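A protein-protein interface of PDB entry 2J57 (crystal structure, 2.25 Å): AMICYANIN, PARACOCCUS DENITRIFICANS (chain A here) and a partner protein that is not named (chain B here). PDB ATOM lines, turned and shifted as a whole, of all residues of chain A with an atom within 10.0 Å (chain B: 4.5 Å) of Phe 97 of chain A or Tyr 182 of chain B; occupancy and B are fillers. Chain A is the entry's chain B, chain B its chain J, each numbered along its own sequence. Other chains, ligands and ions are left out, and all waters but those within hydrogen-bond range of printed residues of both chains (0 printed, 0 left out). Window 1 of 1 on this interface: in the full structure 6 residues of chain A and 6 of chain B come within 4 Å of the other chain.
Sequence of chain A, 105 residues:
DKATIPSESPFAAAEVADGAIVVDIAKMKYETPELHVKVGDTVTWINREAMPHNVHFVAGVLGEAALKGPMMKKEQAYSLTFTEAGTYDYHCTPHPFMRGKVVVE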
ATOM      1  N   ILE A  25     -25.423   5.564  19.023  1.00  0.00           N
ATOM      2  CA  ILE A  25     -24.805   6.324  20.122  1.00  0.00           C
ATOM      3  C   ILE A  25     -25.659   6.057  21.343  1.00  0.00           C
ATOM      4  O   ILE A  25     -26.836   6.252  21.304  1.00  0.00           O
ATOM      5  CB  ILE A  25     -24.721   7.896  19.863  1.00  0.00           C
ATOM      6  CG1 ILE A  25     -24.071   8.244  18.493  1.00  0.00           C
ATOM      7  CG2 ILE A  25     -23.923   8.604  20.958  1.00  0.00           C
ATOM      8  CD1 ILE A  25     -24.113   9.774  18.127  1.00  0.00           C
ATOM      9  N   ALA A  26     -25.067   5.565  22.419  1.00  0.00           N
ATOM     10  CA  ALA A  26     -25.817   5.044  23.575  1.00  0.00           C
ATOM     11  C   ALA A  26     -24.809   5.030  24.671  1.00  0.00           C
ATOM     12  O   ALA A  26     -23.639   4.876  24.375  1.00  0.00           O
ATOM     13  CB  ALA A  26     -26.377   3.582  23.330  1.00  0.00           C
ATOM     14  N   LYS A  27     -25.260   5.233  25.912  1.00  0.00           N
ATOM     15  CA  LYS A  27     -24.389   5.321  27.071  1.00  0.00           C
ATOM     16  C   LYS A  27     -23.060   6.035  26.770  1.00  0.00           C
ATOM     17  O   LYS A  27     -21.957   5.529  27.111  1.00  0.00           O
ATOM     18  CB  LYS A  27     -24.134   3.934  27.703  1.00  0.00           C
ATOM     19  CG  LYS A  27     -25.356   3.071  27.982  1.00  0.00           C
ATOM     20  CD  LYS A  27     -25.303   1.846  27.097  1.00  0.00           C
ATOM     21  CE  LYS A  27     -25.943   0.573  27.793  1.00  0.00           C
ATOM     22  NZ  LYS A  27     -25.200  -0.761  27.564  1.00  0.00           N
ATOM     23  N   MET A  28     -23.146   7.223  26.163  1.00  0.00           N
ATOM     24  CA  MET A  28     -21.981   8.101  26.046  1.00  0.00           C
ATOM     25  C   MET A  28     -20.858   7.514  25.170  1.00  0.00           C
ATOM     26  O   MET A  28     -19.684   7.859  25.336  1.00  0.00           O
ATOM     27  CB  MET A  28     -21.458   8.525  27.432  1.00  0.00           C
ATOM     28  CG  MET A  28     -22.537   9.155  28.380  1.00  0.00           C
ATOM     29  SD  MET A  28     -23.379  10.730  27.834  1.00  0.00           S
ATOM     30  CE  MET A  28     -21.977  11.844  27.577  1.00  0.00           C
ATOM     31  N   LYS A  29     -21.227   6.635  24.236  1.00  0.00           N
ATOM     32  CA  LYS A  29     -20.256   6.011  23.408  1.00  0.00           C
ATOM     33  C   LYS A  29     -20.759   5.959  21.977  1.00  0.00           C
ATOM     34  O   LYS A  29     -21.909   5.647  21.720  1.00  0.00           O
ATOM     35  CB  LYS A  29     -19.934   4.562  23.925  1.00  0.00           C
ATOM     36  CG  LYS A  29     -19.393   4.503  25.383  1.00  0.00           C
ATOM     37  CD  LYS A  29     -19.281   3.056  25.976  1.00  0.00           C
ATOM     38  CE  LYS A  29     -18.265   3.073  27.160  1.00  0.00           C
ATOM     39  NZ  LYS A  29     -17.786   1.741  27.741  1.00  0.00           N
ATOM     40  N   TYR A  30     -19.870   6.221  21.042  1.00  0.00           N
ATOM     41  CA  TYR A  30     -20.099   5.788  19.692  1.00  0.00           C
ATOM     42  C   TYR A  30     -20.082   4.265  19.633  1.00  0.00           C
ATOM     43  O   TYR A  30     -19.332   3.575  20.375  1.00  0.00           O
ATOM     44  CB  TYR A  30     -19.050   6.405  18.752  1.00  0.00           C
ATOM     45  CG  TYR A  30     -19.078   7.958  18.696  1.00  0.00           C
ATOM     46  CD1 TYR A  30     -20.184   8.640  18.188  1.00  0.00           C
ATOM     47  CD2 TYR A  30     -18.000   8.713  19.150  1.00  0.00           C
ATOM     48  CE1 TYR A  30     -20.186  10.032  18.127  1.00  0.00           C
ATOM     49  CE2 TYR A  30     -18.011  10.054  19.100  1.00  0.00           C
ATOM     50  CZ  TYR A  30     -19.077  10.705  18.569  1.00  0.00           C
ATOM     51  OH  TYR A  30     -19.064  12.045  18.540  1.00  0.00           O
ATOM     52  N   PRO A  33     -15.388   2.209  17.553  1.00  0.00           N
ATOM     53  CA  PRO A  33     -14.297   3.205  17.667  1.00  0.00           C
ATOM     54  C   PRO A  33     -13.842   3.609  16.290  1.00  0.00           C
ATOM     55  O   PRO A  33     -13.251   4.668  16.114  1.00  0.00           O
ATOM     56  CB  PRO A  33     -13.157   2.405  18.339  1.00  0.00           C
ATOM     57  CG  PRO A  33     -13.422   0.962  17.909  1.00  0.00           C
ATOM     58  CD  PRO A  33     -14.962   0.868  18.008  1.00  0.00           C
ATOM     59  N   GLU A  49     -30.118   7.832  22.684  1.00  0.00           N
ATOM     60  CA  GLU A  49     -30.400   8.240  24.062  1.00  0.00           C
ATOM     61  C   GLU A  49     -30.782   9.701  24.158  1.00  0.00           C
ATOM     62  O   GLU A  49     -30.689  10.430  23.155  1.00  0.00           O
ATOM     63  CB  GLU A  49     -29.202   7.958  24.977  1.00  0.00           C
ATOM     64  CG  GLU A  49     -27.834   8.536  24.471  1.00  0.00           C
ATOM     65  CD  GLU A  49     -26.774   8.434  25.560  1.00  0.00           C
ATOM     66  OE1 GLU A  49     -27.151   8.183  26.718  1.00  0.00           O
ATOM     67  OE2 GLU A  49     -25.580   8.597  25.279  1.00  0.00           O
ATOM     68  N   MET A  51     -29.487  12.174  26.064  1.00  0.00           N
ATOM     69  CA  MET A  51     -28.321  13.033  26.086  1.00  0.00           C
ATOM     70  C   MET A  51     -27.999  13.398  24.649  1.00  0.00           C
ATOM     71  O   MET A  51     -27.822  12.492  23.831  1.00  0.00           O
ATOM     72  CB  MET A  51     -27.164  12.294  26.717  1.00  0.00           C
ATOM     73  CG  MET A  51     -25.863  13.052  26.632  1.00  0.00           C
ATOM     74  SD  MET A  51     -25.876  14.555  27.616  1.00  0.00           S
ATOM     75  CE  MET A  51     -25.654  13.885  29.268  1.00  0.00           C
ATOM     76  N   PRO A  52     -28.011  14.713  24.303  1.00  0.00           N
ATOM     77  CA  PRO A  52     -27.587  15.110  22.944  1.00  0.00           C
ATOM     78  C   PRO A  52     -26.107  14.862  22.610  1.00  0.00           C
ATOM     79  O   PRO A  52     -25.215  15.074  23.439  1.00  0.00           O
ATOM     80  CB  PRO A  52     -27.943  16.629  22.891  1.00  0.00           C
ATOM     81  CG  PRO A  52     -29.006  16.775  23.960  1.00  0.00           C
ATOM     82  CD  PRO A  52     -28.456  15.891  25.071  1.00  0.00           C
ATOM     83  N   HIS A  53     -25.883  14.430  21.372  1.00  0.00           N
ATOM     84  CA  HIS A  53     -24.596  14.071  20.867  1.00  0.00           C
ATOM     85  C   HIS A  53     -24.496  14.606  19.451  1.00  0.00           C
ATOM     86  O   HIS A  53     -25.514  14.751  18.775  1.00  0.00           O
ATOM     87  CB  HIS A  53     -24.426  12.495  20.857  1.00  0.00           C
ATOM     88  CG  HIS A  53     -24.402  11.861  22.229  1.00  0.00           C
ATOM     89  ND1 HIS A  53     -23.567  12.289  23.243  1.00  0.00           N
ATOM     90  CD2 HIS A  53     -25.146  10.860  22.768  1.00  0.00           C
ATOM     91  CE1 HIS A  53     -23.798  11.587  24.341  1.00  0.00           C
ATOM     92  NE2 HIS A  53     -24.728  10.694  24.068  1.00  0.00           N
ATOM     93  N   ASN A  54     -23.271  14.839  18.963  1.00  0.00           N
ATOM     94  CA  ASN A  54     -23.086  15.142  17.555  1.00  0.00           C
ATOM     95  C   ASN A  54     -21.819  14.452  17.080  1.00  0.00           C
ATOM     96  O   ASN A  54     -21.289  13.582  17.784  1.00  0.00           O
ATOM     97  CB  ASN A  54     -22.995  16.676  17.306  1.00  0.00           C
ATOM     98  CG  ASN A  54     -21.672  17.303  17.826  1.00  0.00           C
ATOM     99  OD1 ASN A  54     -21.055  16.793  18.748  1.00  0.00           O
ATOM    100  ND2 ASN A  54     -21.230  18.366  17.187  1.00  0.00           N
ATOM    101  N   TYR A  90     -13.089  12.127  14.607  1.00  0.00           N
ATOM    102  CA  TYR A  90     -14.158  12.976  15.099  1.00  0.00           C
ATOM    103  C   TYR A  90     -14.332  12.795  16.596  1.00  0.00           C
ATOM    104  O   TYR A  90     -13.834  11.808  17.193  1.00  0.00           O
ATOM    105  CB  TYR A  90     -15.476  12.729  14.329  1.00  0.00           C
ATOM    106  CG  TYR A  90     -16.083  11.319  14.440  1.00  0.00           C
ATOM    107  CD1 TYR A  90     -15.743  10.295  13.542  1.00  0.00           C
ATOM    108  CD2 TYR A  90     -17.067  11.028  15.421  1.00  0.00           C
ATOM    109  CE1 TYR A  90     -16.335   8.977  13.655  1.00  0.00           C
ATOM    110  CE2 TYR A  90     -17.649   9.749  15.520  1.00  0.00           C
ATOM    111  CZ  TYR A  90     -17.283   8.734  14.660  1.00  0.00           C
ATOM    112  OH  TYR A  90     -17.956   7.533  14.785  1.00  0.00           O
ATOM    113  N   HIS A  91     -14.993  13.768  17.217  1.00  0.00           N
ATOM    114  CA  HIS A  91     -15.446  13.661  18.610  1.00  0.00           C
ATOM    115  C   HIS A  91     -16.795  14.308  18.675  1.00  0.00           C
ATOM    116  O   HIS A  91     -17.283  14.857  17.675  1.00  0.00           O
ATOM    117  CB  HIS A  91     -14.455  14.296  19.615  1.00  0.00           C
ATOM    118  CG  HIS A  91     -14.295  15.774  19.445  1.00  0.00           C
ATOM    119  ND1 HIS A  91     -13.626  16.333  18.380  1.00  0.00           N
ATOM    120  CD2 HIS A  91     -14.733  16.810  20.196  1.00  0.00           C
ATOM    121  CE1 HIS A  91     -13.662  17.647  18.475  1.00  0.00           C
ATOM    122  NE2 HIS A  91     -14.347  17.960  19.560  1.00  0.00           N
ATOM    123  N   CYS A  92     -17.430  14.162  19.818  1.00  0.00           N
ATOM    124  CA  CYS A  92     -18.669  14.854  20.158  1.00  0.00           C
ATOM    125  C   CYS A  92     -18.284  16.148  20.872  1.00  0.00           C
ATOM    126  O   CYS A  92     -17.554  16.098  21.858  1.00  0.00           O
ATOM    127  CB  CYS A  92     -19.487  13.937  21.066  1.00  0.00           C
ATOM    128  SG  CYS A  92     -21.022  14.641  21.573  1.00  0.00           S
ATOM    129  N   THR A  93     -18.734  17.305  20.346  1.00  0.00           N
ATOM    130  CA  THR A  93     -18.294  18.622  20.765  1.00  0.00           C
ATOM    131  C   THR A  93     -18.266  18.859  22.284  1.00  0.00           C
ATOM    132  O   THR A  93     -17.204  19.255  22.848  1.00  0.00           O
ATOM    133  CB  THR A  93     -19.098  19.700  20.051  1.00  0.00           C
ATOM    134  OG1 THR A  93     -18.990  19.499  18.636  1.00  0.00           O
ATOM    135  CG2 THR A  93     -18.589  21.069  20.369  1.00  0.00           C
ATOM    136  N   PRO A  94     -19.436  18.650  22.966  1.00  0.00           N
ATOM    137  CA  PRO A  94     -19.472  18.821  24.457  1.00  0.00           C
ATOM    138  C   PRO A  94     -18.721  17.711  25.173  1.00  0.00           C
ATOM    139  O   PRO A  94     -18.406  17.839  26.362  1.00  0.00           O
ATOM    140  CB  PRO A  94     -20.947  18.673  24.768  1.00  0.00           C
ATOM    141  CG  PRO A  94     -21.496  17.782  23.639  1.00  0.00           C
ATOM    142  CD  PRO A  94     -20.770  18.299  22.417  1.00  0.00           C
ATOM    143  N   HIS A  95     -18.439  16.606  24.453  1.00  0.00           N
ATOM    144  CA  HIS A  95     -17.928  15.385  25.083  1.00  0.00           C
ATOM    145  C   HIS A  95     -16.663  14.885  24.376  1.00  0.00           C
ATOM    146  O   HIS A  95     -16.749  13.926  23.628  1.00  0.00           O
ATOM    147  CB  HIS A  95     -18.989  14.281  25.032  1.00  0.00           C
ATOM    148  CG  HIS A  95     -20.322  14.706  25.524  1.00  0.00           C
ATOM    149  ND1 HIS A  95     -21.487  14.154  25.051  1.00  0.00           N
ATOM    150  CD2 HIS A  95     -20.678  15.606  26.473  1.00  0.00           C
ATOM    151  CE1 HIS A  95     -22.510  14.715  25.681  1.00  0.00           C
ATOM    152  NE2 HIS A  95     -22.041  15.603  26.541  1.00  0.00           N
ATOM    153  N   PRO A  96     -15.521  15.576  24.566  1.00  0.00           N
ATOM    154  CA  PRO A  96     -14.172  15.250  23.998  1.00  0.00           C
ATOM    155  C   PRO A  96     -13.735  13.780  24.124  1.00  0.00           C
ATOM    156  O   PRO A  96     -12.984  13.292  23.288  1.00  0.00           O
ATOM    157  CB  PRO A  96     -13.237  16.146  24.826  1.00  0.00           C
ATOM    158  CG  PRO A  96     -14.112  17.411  25.076  1.00  0.00           C
ATOM    159  CD  PRO A  96     -15.484  16.832  25.366  1.00  0.00           C
ATOM    160  N   PHE A  97     -14.203  13.123  25.189  1.00  0.00           N
ATOM    161  CA  PHE A  97     -13.980  11.720  25.487  1.00  0.00           C
ATOM    162  C   PHE A  97     -14.751  10.727  24.576  1.00  0.00           C
ATOM    163  O   PHE A  97     -14.403   9.541  24.579  1.00  0.00           O
ATOM    164  CB  PHE A  97     -14.284  11.425  26.962  1.00  0.00           C
ATOM    165  CG  PHE A  97     -15.696  11.735  27.365  1.00  0.00           C
ATOM    166  CD1 PHE A  97     -16.695  10.748  27.297  1.00  0.00           C
ATOM    167  CD2 PHE A  97     -16.048  12.998  27.828  1.00  0.00           C
ATOM    168  CE1 PHE A  97     -18.008  11.053  27.652  1.00  0.00           C
ATOM    169  CE2 PHE A  97     -17.397  13.288  28.184  1.00  0.00           C
ATOM    170  CZ  PHE A  97     -18.349  12.323  28.088  1.00  0.00           C
ATOM    171  N   MET A  98     -15.771  11.183  23.839  1.00  0.00           N
ATOM    172  CA  MET A  98     -16.418  10.396  22.811  1.00  0.00           C
ATOM    173  C   MET A  98     -15.661  10.670  21.531  1.00  0.00           C
ATOM    174  O   MET A  98     -15.694  11.785  21.011  1.00  0.00           O
ATOM    175  CB  MET A  98     -17.915  10.777  22.659  1.00  0.00           C
ATOM    176  CG  MET A  98     -18.714  10.471  23.882  1.00  0.00           C
ATOM    177  SD  MET A  98     -20.453  10.932  23.885  1.00  0.00           S
ATOM    178  CE  MET A  98     -20.994   9.975  22.467  1.00  0.00           C
ATOM    179  N   ARG A  99     -14.946   9.657  21.042  1.00  0.00           N
ATOM    180  CA  ARG A  99     -14.089   9.764  19.845  1.00  0.00           C
ATOM    181  C   ARG A  99     -14.322   8.646  18.843  1.00  0.00           C
ATOM    182  O   ARG A  99     -14.389   7.467  19.197  1.00  0.00           O
ATOM    183  CB  ARG A  99     -12.667   9.668  20.278  1.00  0.00           C
ATOM    184  CG  ARG A  99     -12.092  10.949  20.707  1.00  0.00           C
ATOM    185  CD  ARG A  99     -10.694  10.703  21.174  1.00  0.00           C
ATOM    186  NE  ARG A  99     -10.703  11.212  22.515  1.00  0.00           N
ATOM    187  CZ  ARG A  99     -10.427  10.515  23.602  1.00  0.00           C
ATOM    188  NH1 ARG A  99     -10.008   9.277  23.534  1.00  0.00           N
ATOM    189  NH2 ARG A  99     -10.527  11.109  24.771  1.00  0.00           N
ATOM    190  N   GLY A 100     -14.416   8.987  17.578  1.00  0.00           N
ATOM    191  CA  GLY A 100     -14.541   7.948  16.617  1.00  0.00           C
ATOM    192  C   GLY A 100     -13.600   8.201  15.489  1.00  0.00           C
ATOM    193  O   GLY A 100     -12.846   9.155  15.508  1.00  0.00           O
ATOM    194  N   MET B 141      -5.680  22.006  37.910  1.00  0.00           N
ATOM    195  CA  MET B 141      -5.747  22.043  36.413  1.00  0.00           C
ATOM    196  C   MET B 141      -4.514  22.686  35.797  1.00  0.00           C
ATOM    197  O   MET B 141      -4.386  22.751  34.585  1.00  0.00           O
ATOM    198  CB  MET B 141      -7.002  22.739  35.893  1.00  0.00           C
ATOM    199  CG  MET B 141      -8.246  21.895  35.961  1.00  0.00           C
ATOM    200  SD  MET B 141      -8.182  20.364  34.964  1.00  0.00           S
ATOM    201  CE  MET B 141      -9.719  19.596  35.470  1.00  0.00           C
ATOM    202  N   TYR B 154      -4.062  21.564  31.794  1.00  0.00           N
ATOM    203  CA  TYR B 154      -5.035  20.668  31.192  1.00  0.00           C
ATOM    204  C   TYR B 154      -5.733  21.391  30.004  1.00  0.00           C
ATOM    205  O   TYR B 154      -6.088  22.566  30.121  1.00  0.00           O
ATOM    206  CB  TYR B 154      -6.041  20.180  32.225  1.00  0.00           C
ATOM    207  CG  TYR B 154      -6.987  19.142  31.664  1.00  0.00           C
ATOM    208  CD1 TYR B 154      -6.505  17.899  31.216  1.00  0.00           C
ATOM    209  CD2 TYR B 154      -8.346  19.400  31.546  1.00  0.00           C
ATOM    210  CE1 TYR B 154      -7.371  16.941  30.653  1.00  0.00           C
ATOM    211  CE2 TYR B 154      -9.238  18.438  31.007  1.00  0.00           C
ATOM    212  CZ  TYR B 154      -8.755  17.204  30.564  1.00  0.00           C
ATOM    213  OH  TYR B 154      -9.628  16.244  30.004  1.00  0.00           O
ATOM    214  N   PHE B 156      -9.125  20.508  27.652  1.00  0.00           N
ATOM    215  CA  PHE B 156     -10.293  19.639  27.663  1.00  0.00           C
ATOM    216  C   PHE B 156     -10.765  19.307  26.256  1.00  0.00           C
ATOM    217  O   PHE B 156     -10.997  18.139  25.917  1.00  0.00           O
ATOM    218  CB  PHE B 156     -11.353  20.296  28.522  1.00  0.00           C
ATOM    219  CG  PHE B 156     -12.735  19.751  28.367  1.00  0.00           C
ATOM    220  CD1 PHE B 156     -13.113  18.605  29.059  1.00  0.00           C
ATOM    221  CD2 PHE B 156     -13.718  20.489  27.627  1.00  0.00           C
ATOM    222  CE1 PHE B 156     -14.396  18.119  28.966  1.00  0.00           C
ATOM    223  CE2 PHE B 156     -15.015  20.027  27.521  1.00  0.00           C
ATOM    224  CZ  PHE B 156     -15.357  18.832  28.192  1.00  0.00           C
ATOM    225  N   ASP B 180      -8.916   9.777  28.930  1.00  0.00           N
ATOM    226  CA  ASP B 180     -10.042  10.621  29.327  1.00  0.00           C
ATOM    227  C   ASP B 180     -10.031  10.964  30.808  1.00  0.00           C
ATOM    228  O   ASP B 180     -10.884  10.517  31.553  1.00  0.00           O
ATOM    229  CB  ASP B 180     -11.356  10.025  28.804  1.00  0.00           C
ATOM    230  CG  ASP B 180     -11.474  10.197  27.288  1.00  0.00           C
ATOM    231  OD1 ASP B 180     -11.228  11.370  26.860  1.00  0.00           O
ATOM    232  OD2 ASP B 180     -11.750   9.211  26.512  1.00  0.00           O
ATOM    233  N   CYS B 181      -9.029  11.757  31.206  1.00  0.00           N
ATOM    234  CA  CYS B 181      -8.705  12.046  32.618  1.00  0.00           C
ATOM    235  C   CYS B 181      -8.584  13.571  32.864  1.00  0.00           C
ATOM    236  O   CYS B 181      -8.631  14.346  31.906  1.00  0.00           O
ATOM    237  CB  CYS B 181      -7.420  11.295  33.008  1.00  0.00           C
ATOM    238  SG  CYS B 181      -7.467   9.527  32.432  1.00  0.00           S
ATOM    239  N   TYR B 182      -8.449  13.980  34.142  1.00  0.00           N
ATOM    240  CA  TYR B 182      -8.722  15.401  34.583  1.00  0.00           C
ATOM    241  C   TYR B 182      -7.857  15.712  35.771  1.00  0.00           C
ATOM    242  O   TYR B 182      -7.602  14.802  36.545  1.00  0.00           O
ATOM    243  CB  TYR B 182     -10.223  15.628  34.951  1.00  0.00           C
ATOM    244  CG  TYR B 182     -11.091  15.252  33.813  1.00  0.00           C
ATOM    245  CD1 TYR B 182     -11.371  13.874  33.542  1.00  0.00           C
ATOM    246  CD2 TYR B 182     -11.595  16.233  32.920  1.00  0.00           C
ATOM    247  CE1 TYR B 182     -12.108  13.488  32.436  1.00  0.00           C
ATOM    248  CE2 TYR B 182     -12.376  15.838  31.816  1.00  0.00           C
ATOM    249  CZ  TYR B 182     -12.588  14.475  31.576  1.00  0.00           C
ATOM    250  OH  TYR B 182     -13.341  14.096  30.512  1.00  0.00           O
ATOM    251  N   HIS B 183      -7.427  16.974  35.936  1.00  0.00           N
ATOM    252  CA  HIS B 183      -6.471  17.355  37.002  1.00  0.00           C
ATOM    253  C   HIS B 183      -5.082  16.710  36.775  1.00  0.00           C
ATOM    254  O   HIS B 183      -4.964  15.748  35.991  1.00  0.00           O
ATOM    255  CB  HIS B 183      -6.954  16.936  38.352  1.00  0.00           C
ATOM    256  CG  HIS B 183      -8.201  17.625  38.799  1.00  0.00           C
ATOM    257  ND1 HIS B 183      -9.458  17.130  38.531  1.00  0.00           N
ATOM    258  CD2 HIS B 183      -8.383  18.736  39.537  1.00  0.00           C
ATOM    259  CE1 HIS B 183     -10.366  17.926  39.057  1.00  0.00           C
ATOM    260  NE2 HIS B 183      -9.743  18.904  39.684  1.00  0.00           N
ATOM    261  N   ILE B 184      -4.066  17.298  37.413  1.00  0.00           N
ATOM    262  CA  ILE B 184      -2.673  17.093  37.106  1.00  0.00           C
ATOM    263  C   ILE B 184      -1.944  17.196  38.437  1.00  0.00           C
ATOM    264  O   ILE B 184      -1.872  18.300  39.051  1.00  0.00           O
ATOM    265  CB  ILE B 184      -2.100  18.133  36.077  1.00  0.00           C
ATOM    266  CG1 ILE B 184      -2.833  18.074  34.720  1.00  0.00           C
ATOM    267  CG2 ILE B 184      -0.657  17.912  35.854  1.00  0.00           C
ATOM    268  CD1 ILE B 184      -2.688  19.282  33.937  1.00  0.00           C
ATOM    269  N   MET B 194      -3.405  11.713  36.852  1.00  0.00           N
ATOM    270  CA  MET B 194      -4.645  12.360  36.476  1.00  0.00           C
ATOM    271  C   MET B 194      -5.722  11.501  37.073  1.00  0.00           C
ATOM    272  O   MET B 194      -5.448  10.389  37.443  1.00  0.00           O
ATOM    273  CB  MET B 194      -4.782  12.413  34.962  1.00  0.00           C
ATOM    274  CG  MET B 194      -3.533  12.923  34.237  1.00  0.00           C
ATOM    275  SD  MET B 194      -4.001  13.326  32.582  1.00  0.00           S
ATOM    276  CE  MET B 194      -4.851  14.898  32.968  1.00  0.00           C
ATOM    277  N   HIS B 195      -6.934  12.025  37.212  1.00  0.00           N
ATOM    278  CA  HIS B 195      -8.072  11.211  37.584  1.00  0.00           C
ATOM    279  C   HIS B 195      -8.979  10.923  36.359  1.00  0.00           C
ATOM    280  O   HIS B 195      -9.314  11.880  35.588  1.00  0.00           O
ATOM    281  CB  HIS B 195      -8.826  11.910  38.668  1.00  0.00           C
ATOM    282  CG  HIS B 195     -10.114  11.241  39.008  1.00  0.00           C
ATOM    283  ND1 HIS B 195     -11.331  11.895  38.963  1.00  0.00           N
ATOM    284  CD2 HIS B 195     -10.381   9.959  39.346  1.00  0.00           C
ATOM    285  CE1 HIS B 195     -12.290  11.044  39.282  1.00  0.00           C
ATOM    286  NE2 HIS B 195     -11.740   9.861  39.509  1.00  0.00           N
ATOM    287  N   ARG B 197     -12.468   9.310  34.023  1.00  0.00           N
ATOM    288  CA  ARG B 197     -13.940   9.041  33.913  1.00  0.00           C
ATOM    289  C   ARG B 197     -14.312   7.649  34.482  1.00  0.00           C
ATOM    290  O   ARG B 197     -15.058   7.549  35.475  1.00  0.00           O
ATOM    291  CB  ARG B 197     -14.508   9.227  32.457  1.00  0.00           C
ATOM    292  CG  ARG B 197     -15.991   8.798  32.317  1.00  0.00           C
ATOM    293  CD  ARG B 197     -16.617   8.888  30.892  1.00  0.00           C
ATOM    294  NE  ARG B 197     -17.211  10.206  30.831  1.00  0.00           N
ATOM    295  CZ  ARG B 197     -18.490  10.514  30.884  1.00  0.00           C
ATOM    296  NH1 ARG B 197     -18.750  11.801  30.879  1.00  0.00           N
ATOM    297  NH2 ARG B 197     -19.485   9.620  30.855  1.00  0.00           N
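NH2 of Arg 99 of chain A lies within salt-bridge range of OD2 of Asp 180 of chain B.
O of Phe 97 of chain A sits close to OD2 of Asp 180 of chain B.
OE2 of Glu 49 of chain A sits at hydrogen-bond distance from N of Met 28 of chain A (2.9 Å).
The backbone carbonyl oxygen of Pro 96 of chain A lies within hydrogen-bond range of the guanidinium group of Arg 99 of chain A, 3.2 Å away.
The backbone NH (N) of Arg 197 of chain B lies within hydrogen-bond range of the backbone carbonyl oxygen (O) of Asp 180 of chain B (3.2 Å).
The backbone carbonyl oxygen (O) of His 195 of chain B lies within hydrogen-bond range of the backbone NH (N) of Tyr 182 of chain B.
Among the printed residues, pairs that only touch across the chains: Met 28 of chain A with Arg 197 of chain B (3.96 Å), Pro 94 of chain A with Phe 156 of chain B (3.7 Å), Pro 96 of chain A with Phe 156 of chain B (3.2 Å), Phe 97 of chain A with Tyr 182 of chain B (3.97 Å) and Phe 97 of chain A with Arg 197 of chain B (2.9 Å).
Ala 26 of chain A touches none of the printed residues of chain B.
Of the printed residues of chain B, Met 28 of chain A touches Arg 197.
Printed residues of chain B within 4 Å of Pro 96 of chain A: Phe 156 (3.2 Å).
Printed residues of chain B within 4 Å of Phe 97 of chain A: Asp 180 (3.1 Å), Tyr 182 (3.97 Å) and Arg 197 (2.9 Å).
Of the printed residues of chain B, Arg 99 of chain A touches Asp 180 (2.2 Å).
Of the printed residues of chain A, Asp 180 of chain B touches Phe 97 and Arg 99.
No residue of chain A comes within 4 Å of Cys 181 of chain B.
No residue of chain A comes within 4 Å of Met 194 of chain B.
The nearest printed residue of chain B that does not touch Arg 99 of chain A is Cys 181 of chain B (6.6 Å).
Printed residues of chain A that touch a printed residue of chain B: Met 28, Pro 94, Pro 96, Phe 97 and Arg 99.
Along chain A the printed residues that touch a printed residue of chain B span positions 28 to 99.
Of the 11 printed residues of chain B, 4 touch a printed residue of chain A.
Hydrophobic or aromatic side chains of chain B within 4 Å of the printed part of chain A: Phe 156 and Tyr 182.
Among the printed residues, 7 pairs touch across the chains.
Among the printed residues, Asp or Glu carboxylates within 4 Å of a Lys or Arg side-chain nitrogen of the other chain: Arg 99 of chain A with Asp 180 of chain B.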
